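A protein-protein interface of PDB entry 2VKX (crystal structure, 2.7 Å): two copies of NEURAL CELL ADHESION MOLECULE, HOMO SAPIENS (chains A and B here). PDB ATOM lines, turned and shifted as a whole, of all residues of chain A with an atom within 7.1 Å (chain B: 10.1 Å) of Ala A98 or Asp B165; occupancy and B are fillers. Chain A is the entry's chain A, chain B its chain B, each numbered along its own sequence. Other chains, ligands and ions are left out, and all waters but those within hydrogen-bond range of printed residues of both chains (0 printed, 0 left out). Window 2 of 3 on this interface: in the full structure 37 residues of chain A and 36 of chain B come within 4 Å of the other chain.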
ATOM      1  N   SER A  11      -8.726  14.961  -9.681  1.00  0.00           N
ATOM      2  CA  SER A  11      -8.987  15.204  -8.261  1.00  0.00           C
ATOM      3  C   SER A  11      -7.821  15.056  -7.300  1.00  0.00           C
ATOM      4  O   SER A  11      -6.948  14.215  -7.477  1.00  0.00           O
ATOM      5  CB  SER A  11     -10.115  14.302  -7.766  1.00  0.00           C
ATOM      6  OG  SER A  11      -9.696  12.949  -7.725  1.00  0.00           O
ATOM      7  N   PRO A  12      -7.773  15.914  -6.278  1.00  0.00           N
ATOM      8  CA  PRO A  12      -6.676  15.787  -5.322  1.00  0.00           C
ATOM      9  C   PRO A  12      -7.108  14.591  -4.485  1.00  0.00           C
ATOM     10  O   PRO A  12      -8.284  14.229  -4.509  1.00  0.00           O
ATOM     11  CB  PRO A  12      -6.753  17.089  -4.524  1.00  0.00           C
ATOM     12  CG  PRO A  12      -7.396  18.047  -5.475  1.00  0.00           C
ATOM     13  CD  PRO A  12      -8.460  17.205  -6.118  1.00  0.00           C
ATOM     14  N   SER A  13      -6.183  13.967  -3.765  1.00  0.00           N
ATOM     15  CA  SER A  13      -6.550  12.833  -2.927  1.00  0.00           C
ATOM     16  C   SER A  13      -6.357  13.167  -1.472  1.00  0.00           C
ATOM     17  O   SER A  13      -5.314  13.675  -1.085  1.00  0.00           O
ATOM     18  CB  SER A  13      -5.710  11.619  -3.269  1.00  0.00           C
ATOM     19  OG  SER A  13      -6.192  11.036  -4.460  1.00  0.00           O
ATOM     20  N   ILE A  14      -7.367  12.894  -0.662  1.00  0.00           N
ATOM     21  CA  ILE A  14      -7.238  13.180   0.754  1.00  0.00           C
ATOM     22  C   ILE A  14      -6.569  12.002   1.454  1.00  0.00           C
ATOM     23  O   ILE A  14      -6.979  10.858   1.289  1.00  0.00           O
ATOM     24  CB  ILE A  14      -8.611  13.475   1.385  1.00  0.00           C
ATOM     25  CG1 ILE A  14      -9.194  14.741   0.748  1.00  0.00           C
ATOM     26  CG2 ILE A  14      -8.473  13.627   2.896  1.00  0.00           C
ATOM     27  CD1 ILE A  14     -10.530  15.177   1.302  1.00  0.00           C
ATOM     28  N   VAL A  17      -7.126  13.674   7.763  1.00  0.00           N
ATOM     29  CA  VAL A  17      -8.031  14.705   8.230  1.00  0.00           C
ATOM     30  C   VAL A  17      -7.949  14.652   9.742  1.00  0.00           C
ATOM     31  O   VAL A  17      -8.617  13.847  10.378  1.00  0.00           O
ATOM     32  CB  VAL A  17      -9.495  14.485   7.801  1.00  0.00           C
ATOM     33  CG1 VAL A  17     -10.356  15.598   8.403  1.00  0.00           C
ATOM     34  CG2 VAL A  17      -9.616  14.507   6.277  1.00  0.00           C
ATOM     35  N   VAL A  83     -15.791  16.990   3.962  1.00  0.00           N
ATOM     36  CA  VAL A  83     -14.831  17.899   3.358  1.00  0.00           C
ATOM     37  C   VAL A  83     -14.244  17.314   2.065  1.00  0.00           C
ATOM     38  O   VAL A  83     -14.015  16.109   1.964  1.00  0.00           O
ATOM     39  CB  VAL A  83     -13.689  18.245   4.359  1.00  0.00           C
ATOM     40  CG1 VAL A  83     -12.996  16.988   4.816  1.00  0.00           C
ATOM     41  CG2 VAL A  83     -12.689  19.190   3.715  1.00  0.00           C
ATOM     42  N   ARG A  84     -14.021  18.171   1.072  1.00  0.00           N
ATOM     43  CA  ARG A  84     -13.468  17.732  -0.204  1.00  0.00           C
ATOM     44  C   ARG A  84     -12.635  18.834  -0.862  1.00  0.00           C
ATOM     45  O   ARG A  84     -12.787  20.017  -0.550  1.00  0.00           O
ATOM     46  CB  ARG A  84     -14.592  17.289  -1.135  1.00  0.00           C
ATOM     47  CG  ARG A  84     -15.514  18.397  -1.507  1.00  0.00           C
ATOM     48  CD  ARG A  84     -16.796  17.842  -2.079  1.00  0.00           C
ATOM     49  NE  ARG A  84     -17.686  18.901  -2.551  1.00  0.00           N
ATOM     50  CZ  ARG A  84     -18.889  18.699  -3.074  1.00  0.00           C
ATOM     51  NH1 ARG A  84     -19.374  17.472  -3.196  1.00  0.00           N
ATOM     52  NH2 ARG A  84     -19.595  19.735  -3.495  1.00  0.00           N
ATOM     53  N   LEU A  85     -11.754  18.424  -1.774  1.00  0.00           N
ATOM     54  CA  LEU A  85     -10.857  19.340  -2.467  1.00  0.00           C
ATOM     55  C   LEU A  85     -10.945  19.291  -3.984  1.00  0.00           C
ATOM     56  O   LEU A  85     -11.432  18.319  -4.566  1.00  0.00           O
ATOM     57  CB  LEU A  85      -9.415  19.040  -2.081  1.00  0.00           C
ATOM     58  CG  LEU A  85      -8.923  19.363  -0.684  1.00  0.00           C
ATOM     59  CD1 LEU A  85      -7.632  18.603  -0.431  1.00  0.00           C
ATOM     60  CD2 LEU A  85      -8.716  20.861  -0.546  1.00  0.00           C
ATOM     61  N   ILE A  96     -13.603  17.312  -8.205  1.00  0.00           N
ATOM     62  CA  ILE A  96     -13.466  17.303  -6.749  1.00  0.00           C
ATOM     63  C   ILE A  96     -13.229  15.912  -6.180  1.00  0.00           C
ATOM     64  O   ILE A  96     -13.711  14.910  -6.701  1.00  0.00           O
ATOM     65  CB  ILE A  96     -14.705  17.914  -6.044  1.00  0.00           C
ATOM     66  CG1 ILE A  96     -15.981  17.333  -6.648  1.00  0.00           C
ATOM     67  CG2 ILE A  96     -14.664  19.431  -6.138  1.00  0.00           C
ATOM     68  CD1 ILE A  96     -17.252  17.972  -6.132  1.00  0.00           C
ATOM     69  N   SER A  97     -12.473  15.868  -5.095  1.00  0.00           N
ATOM     70  CA  SER A  97     -12.150  14.617  -4.423  1.00  0.00           C
ATOM     71  C   SER A  97     -13.391  13.966  -3.810  1.00  0.00           C
ATOM     72  O   SER A  97     -14.477  14.549  -3.780  1.00  0.00           O
ATOM     73  CB  SER A  97     -11.136  14.884  -3.305  1.00  0.00           C
ATOM     74  OG  SER A  97     -11.754  15.591  -2.242  1.00  0.00           O
ATOM     75  N   ALA A  98     -13.217  12.742  -3.327  1.00  0.00           N
ATOM     76  CA  ALA A  98     -14.290  12.035  -2.657  1.00  0.00           C
ATOM     77  C   ALA A  98     -14.410  12.772  -1.327  1.00  0.00           C
ATOM     78  O   ALA A  98     -13.402  13.215  -0.756  1.00  0.00           O
ATOM     79  CB  ALA A  98     -13.911  10.594  -2.436  1.00  0.00           C
ATOM     80  N   ALA A  99     -15.639  12.911  -0.841  1.00  0.00           N
ATOM     81  CA  ALA A  99     -15.905  13.628   0.399  1.00  0.00           C
ATOM     82  C   ALA A  99     -15.562  12.893   1.694  1.00  0.00           C
ATOM     83  O   ALA A  99     -16.288  12.010   2.138  1.00  0.00           O
ATOM     84  CB  ALA A  99     -17.358  14.051   0.428  1.00  0.00           C
ATOM     85  N   SER A 100     -14.461  13.287   2.311  1.00  0.00           N
ATOM     86  CA  SER A 100     -14.021  12.695   3.565  1.00  0.00           C
ATOM     87  C   SER A 100     -14.931  13.218   4.686  1.00  0.00           C
ATOM     88  O   SER A 100     -15.365  14.365   4.649  1.00  0.00           O
ATOM     89  CB  SER A 100     -12.568  13.088   3.807  1.00  0.00           C
ATOM     90  OG  SER A 100     -12.070  12.488   4.971  1.00  0.00           O
ATOM     91  N   GLU A 101     -15.229  12.379   5.671  1.00  0.00           N
ATOM     92  CA  GLU A 101     -16.107  12.780   6.762  1.00  0.00           C
ATOM     93  C   GLU A 101     -15.432  12.714   8.124  1.00  0.00           C
ATOM     94  O   GLU A 101     -14.710  11.766   8.427  1.00  0.00           O
ATOM     95  CB  GLU A 101     -17.365  11.919   6.751  1.00  0.00           C
ATOM     96  CG  GLU A 101     -18.392  12.283   7.814  1.00  0.00           C
ATOM     97  CD  GLU A 101     -19.805  11.821   7.460  1.00  0.00           C
ATOM     98  OE1 GLU A 101     -19.964  10.705   6.925  1.00  0.00           O
ATOM     99  OE2 GLU A 101     -20.761  12.573   7.731  1.00  0.00           O
ATOM    100  N   PRO B 113     -12.546   5.306  15.224  1.00  0.00           N
ATOM    101  CA  PRO B 113     -13.385   6.097  14.329  1.00  0.00           C
ATOM    102  C   PRO B 113     -14.847   5.763  14.591  1.00  0.00           C
ATOM    103  O   PRO B 113     -15.152   4.746  15.227  1.00  0.00           O
ATOM    104  CB  PRO B 113     -12.929   5.639  12.951  1.00  0.00           C
ATOM    105  CG  PRO B 113     -12.632   4.179  13.185  1.00  0.00           C
ATOM    106  CD  PRO B 113     -11.868   4.215  14.500  1.00  0.00           C
ATOM    107  N   LYS B 114     -15.749   6.616  14.120  1.00  0.00           N
ATOM    108  CA  LYS B 114     -17.167   6.363  14.290  1.00  0.00           C
ATOM    109  C   LYS B 114     -17.675   5.662  13.035  1.00  0.00           C
ATOM    110  O   LYS B 114     -17.273   5.987  11.918  1.00  0.00           O
ATOM    111  CB  LYS B 114     -17.936   7.667  14.518  1.00  0.00           C
ATOM    112  CG  LYS B 114     -17.974   8.155  15.970  1.00  0.00           C
ATOM    113  CD  LYS B 114     -18.866   9.412  16.110  1.00  0.00           C
ATOM    114  CE  LYS B 114     -20.317   9.135  15.649  1.00  0.00           C
ATOM    115  NZ  LYS B 114     -21.163  10.365  15.455  1.00  0.00           N
ATOM    116  N   LEU B 115     -18.560   4.691  13.224  1.00  0.00           N
ATOM    117  CA  LEU B 115     -19.099   3.949  12.101  1.00  0.00           C
ATOM    118  C   LEU B 115     -20.547   4.303  11.839  1.00  0.00           C
ATOM    119  O   LEU B 115     -21.314   4.526  12.761  1.00  0.00           O
ATOM    120  CB  LEU B 115     -18.989   2.450  12.367  1.00  0.00           C
ATOM    121  CG  LEU B 115     -17.640   1.908  12.839  1.00  0.00           C
ATOM    122  CD1 LEU B 115     -17.767   0.393  12.934  1.00  0.00           C
ATOM    123  CD2 LEU B 115     -16.507   2.304  11.889  1.00  0.00           C
ATOM    124  N   GLU B 116     -20.915   4.348  10.567  1.00  0.00           N
ATOM    125  CA  GLU B 116     -22.280   4.658  10.173  1.00  0.00           C
ATOM    126  C   GLU B 116     -22.664   3.695   9.063  1.00  0.00           C
ATOM    127  O   GLU B 116     -21.933   3.546   8.085  1.00  0.00           O
ATOM    128  CB  GLU B 116     -22.370   6.096   9.664  1.00  0.00           C
ATOM    129  CG  GLU B 116     -23.682   6.432   8.976  1.00  0.00           C
ATOM    130  CD  GLU B 116     -23.632   7.755   8.237  1.00  0.00           C
ATOM    131  OE1 GLU B 116     -23.595   8.819   8.893  1.00  0.00           O
ATOM    132  OE2 GLU B 116     -23.621   7.731   6.993  1.00  0.00           O
ATOM    133  N   GLY B 117     -23.808   3.042   9.216  1.00  0.00           N
ATOM    134  CA  GLY B 117     -24.251   2.102   8.208  1.00  0.00           C
ATOM    135  C   GLY B 117     -25.084   2.755   7.127  1.00  0.00           C
ATOM    136  O   GLY B 117     -25.742   3.773   7.355  1.00  0.00           O
ATOM    137  N   GLN B 118     -25.051   2.153   5.942  1.00  0.00           N
ATOM    138  CA  GLN B 118     -25.793   2.638   4.790  1.00  0.00           C
ATOM    139  C   GLN B 118     -26.092   1.422   3.917  1.00  0.00           C
ATOM    140  O   GLN B 118     -25.381   0.420   3.976  1.00  0.00           O
ATOM    141  CB  GLN B 118     -24.941   3.635   4.005  1.00  0.00           C
ATOM    142  CG  GLN B 118     -25.714   4.529   3.051  1.00  0.00           C
ATOM    143  CD  GLN B 118     -24.796   5.370   2.168  1.00  0.00           C
ATOM    144  OE1 GLN B 118     -23.780   5.899   2.627  1.00  0.00           O
ATOM    145  NE2 GLN B 118     -25.159   5.505   0.899  1.00  0.00           N
ATOM    146  N   LYS B 127     -22.913  -0.740   3.274  1.00  0.00           N
ATOM    147  CA  LYS B 127     -21.840   0.226   3.121  1.00  0.00           C
ATOM    148  C   LYS B 127     -21.550   0.827   4.495  1.00  0.00           C
ATOM    149  O   LYS B 127     -22.421   1.444   5.104  1.00  0.00           O
ATOM    150  CB  LYS B 127     -22.257   1.331   2.146  1.00  0.00           C
ATOM    151  CG  LYS B 127     -21.131   2.284   1.798  1.00  0.00           C
ATOM    152  CD  LYS B 127     -21.581   3.386   0.862  1.00  0.00           C
ATOM    153  CE  LYS B 127     -20.411   4.295   0.520  1.00  0.00           C
ATOM    154  NZ  LYS B 127     -20.832   5.522  -0.214  1.00  0.00           N
ATOM    155  N   VAL B 128     -20.332   0.633   4.989  1.00  0.00           N
ATOM    156  CA  VAL B 128     -19.968   1.159   6.292  1.00  0.00           C
ATOM    157  C   VAL B 128     -19.135   2.421   6.131  1.00  0.00           C
ATOM    158  O   VAL B 128     -17.962   2.365   5.761  1.00  0.00           O
ATOM    159  CB  VAL B 128     -19.189   0.107   7.114  1.00  0.00           C
ATOM    160  CG1 VAL B 128     -18.716   0.710   8.433  1.00  0.00           C
ATOM    161  CG2 VAL B 128     -20.074  -1.101   7.376  1.00  0.00           C
ATOM    162  N   ASN B 129     -19.760   3.560   6.405  1.00  0.00           N
ATOM    163  CA  ASN B 129     -19.104   4.855   6.294  1.00  0.00           C
ATOM    164  C   ASN B 129     -18.260   5.177   7.521  1.00  0.00           C
ATOM    165  O   ASN B 129     -18.682   4.943   8.655  1.00  0.00           O
ATOM    166  CB  ASN B 129     -20.155   5.953   6.129  1.00  0.00           C
ATOM    167  CG  ASN B 129     -20.875   5.877   4.815  1.00  0.00           C
ATOM    168  OD1 ASN B 129     -21.996   6.343   4.697  1.00  0.00           O
ATOM    169  ND2 ASN B 129     -20.231   5.305   3.814  1.00  0.00           N
ATOM    170  N   LEU B 130     -17.076   5.732   7.297  1.00  0.00           N
ATOM    171  CA  LEU B 130     -16.199   6.093   8.404  1.00  0.00           C
ATOM    172  C   LEU B 130     -16.275   7.586   8.717  1.00  0.00           C
ATOM    173  O   LEU B 130     -16.186   8.426   7.819  1.00  0.00           O
ATOM    174  CB  LEU B 130     -14.743   5.757   8.070  1.00  0.00           C
ATOM    175  CG  LEU B 130     -14.401   4.342   7.627  1.00  0.00           C
ATOM    176  CD1 LEU B 130     -12.966   4.325   7.158  1.00  0.00           C
ATOM    177  CD2 LEU B 130     -14.630   3.361   8.767  1.00  0.00           C
ATOM    178  N   ILE B 131     -16.449   7.917   9.988  1.00  0.00           N
ATOM    179  CA  ILE B 131     -16.465   9.311  10.397  1.00  0.00           C
ATOM    180  C   ILE B 131     -15.144   9.444  11.147  1.00  0.00           C
ATOM    181  O   ILE B 131     -15.024   9.019  12.299  1.00  0.00           O
ATOM    182  CB  ILE B 131     -17.654   9.610  11.316  1.00  0.00           C
ATOM    183  CG1 ILE B 131     -18.954   9.467  10.528  1.00  0.00           C
ATOM    184  CG2 ILE B 131     -17.547  11.014  11.868  1.00  0.00           C
ATOM    185  CD1 ILE B 131     -20.189   9.645  11.366  1.00  0.00           C
ATOM    186  N   LYS B 132     -14.147  10.002  10.465  1.00  0.00           N
ATOM    187  CA  LYS B 132     -12.801  10.155  11.015  1.00  0.00           C
ATOM    188  C   LYS B 132     -12.737  10.942  12.311  1.00  0.00           C
ATOM    189  O   LYS B 132     -13.591  11.774  12.585  1.00  0.00           O
ATOM    190  CB  LYS B 132     -11.885  10.784   9.963  1.00  0.00           C
ATOM    191  CG  LYS B 132     -11.703   9.932   8.709  1.00  0.00           C
ATOM    192  CD  LYS B 132     -10.893  10.673   7.656  1.00  0.00           C
ATOM    193  CE  LYS B 132     -10.445   9.762   6.507  1.00  0.00           C
ATOM    194  NZ  LYS B 132     -11.551   9.227   5.652  1.00  0.00           N
ATOM    195  N   GLN B 133     -11.710  10.663  13.108  1.00  0.00           N
ATOM    196  CA  GLN B 133     -11.531  11.317  14.402  1.00  0.00           C
ATOM    197  C   GLN B 133     -10.066  11.505  14.746  1.00  0.00           C
ATOM    198  O   GLN B 133      -9.199  11.020  14.036  1.00  0.00           O
ATOM    199  CB  GLN B 133     -12.219  10.494  15.484  1.00  0.00           C
ATOM    200  CG  GLN B 133     -13.657  10.245  15.148  1.00  0.00           C
ATOM    201  CD  GLN B 133     -14.583  10.530  16.298  1.00  0.00           C
ATOM    202  OE1 GLN B 133     -14.517  11.589  16.922  1.00  0.00           O
ATOM    203  NE2 GLN B 133     -15.466   9.585  16.586  1.00  0.00           N
ATOM    204  N   TYR B 143      -6.538   1.331   8.382  1.00  0.00           N
ATOM    205  CA  TYR B 143      -7.825   1.156   9.034  1.00  0.00           C
ATOM    206  C   TYR B 143      -8.017  -0.353   8.981  1.00  0.00           C
ATOM    207  O   TYR B 143      -8.272  -0.904   7.915  1.00  0.00           O
ATOM    208  CB  TYR B 143      -8.955   1.862   8.277  1.00  0.00           C
ATOM    209  CG  TYR B 143      -9.196   3.269   8.765  1.00  0.00           C
ATOM    210  CD1 TYR B 143      -9.460   3.522  10.111  1.00  0.00           C
ATOM    211  CD2 TYR B 143      -9.088   4.356   7.899  1.00  0.00           C
ATOM    212  CE1 TYR B 143      -9.600   4.825  10.582  1.00  0.00           C
ATOM    213  CE2 TYR B 143      -9.219   5.653   8.356  1.00  0.00           C
ATOM    214  CZ  TYR B 143      -9.472   5.887   9.696  1.00  0.00           C
ATOM    215  OH  TYR B 143      -9.570   7.183  10.147  1.00  0.00           O
ATOM    216  N   VAL B 145     -10.031  -3.511   9.403  1.00  0.00           N
ATOM    217  CA  VAL B 145     -11.433  -3.903   9.444  1.00  0.00           C
ATOM    218  C   VAL B 145     -11.579  -5.421   9.541  1.00  0.00           C
ATOM    219  O   VAL B 145     -10.830  -6.174   8.922  1.00  0.00           O
ATOM    220  CB  VAL B 145     -12.185  -3.441   8.172  1.00  0.00           C
ATOM    221  CG1 VAL B 145     -13.621  -3.949   8.197  1.00  0.00           C
ATOM    222  CG2 VAL B 145     -12.151  -1.948   8.067  1.00  0.00           C
ATOM    223  N   LEU B 160      -7.335  -1.047   5.103  1.00  0.00           N
ATOM    224  CA  LEU B 160      -7.732   0.126   4.332  1.00  0.00           C
ATOM    225  C   LEU B 160      -6.728   1.257   4.485  1.00  0.00           C
ATOM    226  O   LEU B 160      -6.275   1.541   5.594  1.00  0.00           O
ATOM    227  CB  LEU B 160      -9.085   0.639   4.810  1.00  0.00           C
ATOM    228  CG  LEU B 160     -10.290  -0.255   4.573  1.00  0.00           C
ATOM    229  CD1 LEU B 160     -11.503   0.356   5.276  1.00  0.00           C
ATOM    230  CD2 LEU B 160     -10.542  -0.387   3.082  1.00  0.00           C
ATOM    231  N   PRO B 161      -6.359   1.920   3.378  1.00  0.00           N
ATOM    232  CA  PRO B 161      -5.402   3.024   3.506  1.00  0.00           C
ATOM    233  C   PRO B 161      -6.109   4.214   4.175  1.00  0.00           C
ATOM    234  O   PRO B 161      -7.339   4.288   4.182  1.00  0.00           O
ATOM    235  CB  PRO B 161      -4.987   3.283   2.059  1.00  0.00           C
ATOM    236  CG  PRO B 161      -6.213   2.964   1.298  1.00  0.00           C
ATOM    237  CD  PRO B 161      -6.700   1.683   1.965  1.00  0.00           C
ATOM    238  N   SER B 162      -5.335   5.132   4.744  1.00  0.00           N
ATOM    239  CA  SER B 162      -5.893   6.291   5.444  1.00  0.00           C
ATOM    240  C   SER B 162      -6.894   7.150   4.671  1.00  0.00           C
ATOM    241  O   SER B 162      -7.738   7.805   5.276  1.00  0.00           O
ATOM    242  CB  SER B 162      -4.767   7.189   5.921  1.00  0.00           C
ATOM    243  OG  SER B 162      -4.126   7.758   4.800  1.00  0.00           O
ATOM    244  N   GLY B 163      -6.798   7.158   3.346  1.00  0.00           N
ATOM    245  CA  GLY B 163      -7.708   7.965   2.551  1.00  0.00           C
ATOM    246  C   GLY B 163      -9.051   7.317   2.279  1.00  0.00           C
ATOM    247  O   GLY B 163      -9.874   7.847   1.524  1.00  0.00           O
ATOM    248  N   SER B 164      -9.277   6.167   2.894  1.00  0.00           N
ATOM    249  CA  SER B 164     -10.527   5.446   2.718  1.00  0.00           C
ATOM    250  C   SER B 164     -11.641   6.125   3.506  1.00  0.00           C
ATOM    251  O   SER B 164     -11.420   6.633   4.615  1.00  0.00           O
ATOM    252  CB  SER B 164     -10.354   4.000   3.182  1.00  0.00           C
ATOM    253  OG  SER B 164      -9.192   3.435   2.598  1.00  0.00           O
ATOM    254  N   ASP B 165     -12.837   6.138   2.929  1.00  0.00           N
ATOM    255  CA  ASP B 165     -13.982   6.772   3.580  1.00  0.00           C
ATOM    256  C   ASP B 165     -15.073   5.787   3.948  1.00  0.00           C
ATOM    257  O   ASP B 165     -16.012   6.121   4.663  1.00  0.00           O
ATOM    258  CB  ASP B 165     -14.568   7.874   2.689  1.00  0.00           C
ATOM    259  CG  ASP B 165     -13.602   9.023   2.472  1.00  0.00           C
ATOM    260  OD1 ASP B 165     -12.759   9.273   3.361  1.00  0.00           O
ATOM    261  OD2 ASP B 165     -13.695   9.687   1.421  1.00  0.00           O
ATOM    262  N   HIS B 166     -14.956   4.566   3.453  1.00  0.00           N
ATOM    263  CA  HIS B 166     -15.945   3.554   3.765  1.00  0.00           C
ATOM    264  C   HIS B 166     -15.440   2.161   3.458  1.00  0.00           C
ATOM    265  O   HIS B 166     -14.416   1.982   2.793  1.00  0.00           O
ATOM    266  CB  HIS B 166     -17.245   3.806   2.988  1.00  0.00           C
ATOM    267  CG  HIS B 166     -17.083   3.762   1.500  1.00  0.00           C
ATOM    268  ND1 HIS B 166     -17.008   4.900   0.722  1.00  0.00           N
ATOM    269  CD2 HIS B 166     -16.964   2.716   0.646  1.00  0.00           C
ATOM    270  CE1 HIS B 166     -16.851   4.556  -0.544  1.00  0.00           C
ATOM    271  NE2 HIS B 166     -16.820   3.237  -0.617  1.00  0.00           N
ATOM    272  N   VAL B 167     -16.157   1.175   3.979  1.00  0.00           N
ATOM    273  CA  VAL B 167     -15.830  -0.214   3.724  1.00  0.00           C
ATOM    274  C   VAL B 167     -17.111  -0.859   3.195  1.00  0.00           C
ATOM    275  O   VAL B 167     -18.197  -0.697   3.757  1.00  0.00           O
ATOM    276  CB  VAL B 167     -15.288  -0.933   5.003  1.00  0.00           C
ATOM    277  CG1 VAL B 167     -16.052  -0.499   6.229  1.00  0.00           C
ATOM    278  CG2 VAL B 167     -15.372  -2.434   4.824  1.00  0.00           C
ATOM    279  N   MET B 168     -16.977  -1.553   2.075  1.00  0.00           N
ATOM    280  CA  MET B 168     -18.107  -2.206   1.436  1.00  0.00           C
ATOM    281  C   MET B 168     -18.002  -3.707   1.633  1.00  0.00           C
ATOM    282  O   MET B 168     -16.968  -4.309   1.337  1.00  0.00           O
ATOM    283  CB  MET B 168     -18.107  -1.894  -0.063  1.00  0.00           C
ATOM    284  CG  MET B 168     -19.409  -2.217  -0.776  1.00  0.00           C
ATOM    285  SD  MET B 168     -20.675  -1.012  -0.353  1.00  0.00           S
ATOM    286  CE  MET B 168     -19.762   0.549  -0.755  1.00  0.00           C
ATOM    287  N   VAL B 182     -13.748  -2.089  13.377  1.00  0.00           N
ATOM    288  CA  VAL B 182     -12.829  -1.198  12.690  1.00  0.00           C
ATOM    289  C   VAL B 182     -11.887  -0.513  13.683  1.00  0.00           C
ATOM    290  O   VAL B 182     -12.310   0.126  14.653  1.00  0.00           O
ATOM    291  CB  VAL B 182     -13.605  -0.144  11.881  1.00  0.00           C
ATOM    292  CG1 VAL B 182     -12.652   0.679  11.040  1.00  0.00           C
ATOM    293  CG2 VAL B 182     -14.628  -0.824  11.000  1.00  0.00           C
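NZ of Lys B132 lies within hydrogen-bond range of OG of Ser A100 (3.4 Å).
O of Glu A101 sits at hydrogen-bond distance from N of Lys B132.
NZ of Lys B132 is in salt-bridge range of OD1 of Asp B165, 2.6 Å away.
The backbone carbonyl oxygen (O) of Lys B114 lies within hydrogen-bond range of the backbone NH (N) of Ile B131 (2.9 Å).
N of Leu B130 sits at hydrogen-bond distance from O of Asp B165 (2.9 Å).
The side-chain amino group (NZ) of Lys B132 is in hydrogen-bond range of the backbone carbonyl oxygen (O) of Ser B164.
N of Val A83 lies within hydrogen-bond range of O of Ser A100 (2.7 Å).
Among the printed residues, pairs that only touch across the chains: Ile A14 with Gly B163 (3.2 Å), Ala A98 with Asp B165 (3.97 Å), Ala A99 with Asp B165 (3.6 Å), Ser A100 with Asp B165 (3.7 Å), Glu A101 with Leu B130 (3.7 Å) and Glu A101 with Ile B131 (3.6 Å).
Pro A12 touches none of the printed residues of chain B.
No residue of chain B comes within 4 Å of Ser A97.
Ala A99 touches one residue of chain B.
Ser A100 touches just these residues of chain B: Lys B132 (3.4 Å) and Asp B165 (3.7 Å).
Of the printed residues of chain A, Ile B131 touches Glu A101 (3.6 Å).
Of the printed residues of chain A, Gly B163 touches Ile A14 (3.2 Å).
Asp B165 touches three residues of chain A.
The nearest residue of chain B that does not touch Ala A98 is Gly B163 (6.3 Å).
The nearest residue of chain A that does not touch Asp B165 is Glu A101 (4.6 Å).
Hydrophobic or aromatic side chains of chain A that line the printed part of chain B: Ala A98.
Hydrophobic or aromatic side chains of chain B that line the printed part of chain A: Ile B131.
Among the printed residues, 8 pairs touch across the chains.
Among the printed residues, no Asp or Glu carboxylate lies within 4 Å of a Lys or Arg side-chain nitrogen of the other chain.
No position is printed for both chains.
Of the 8 pairs that touch across the chains among the printed residues, none has its exchanged pair printed and touching as well.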
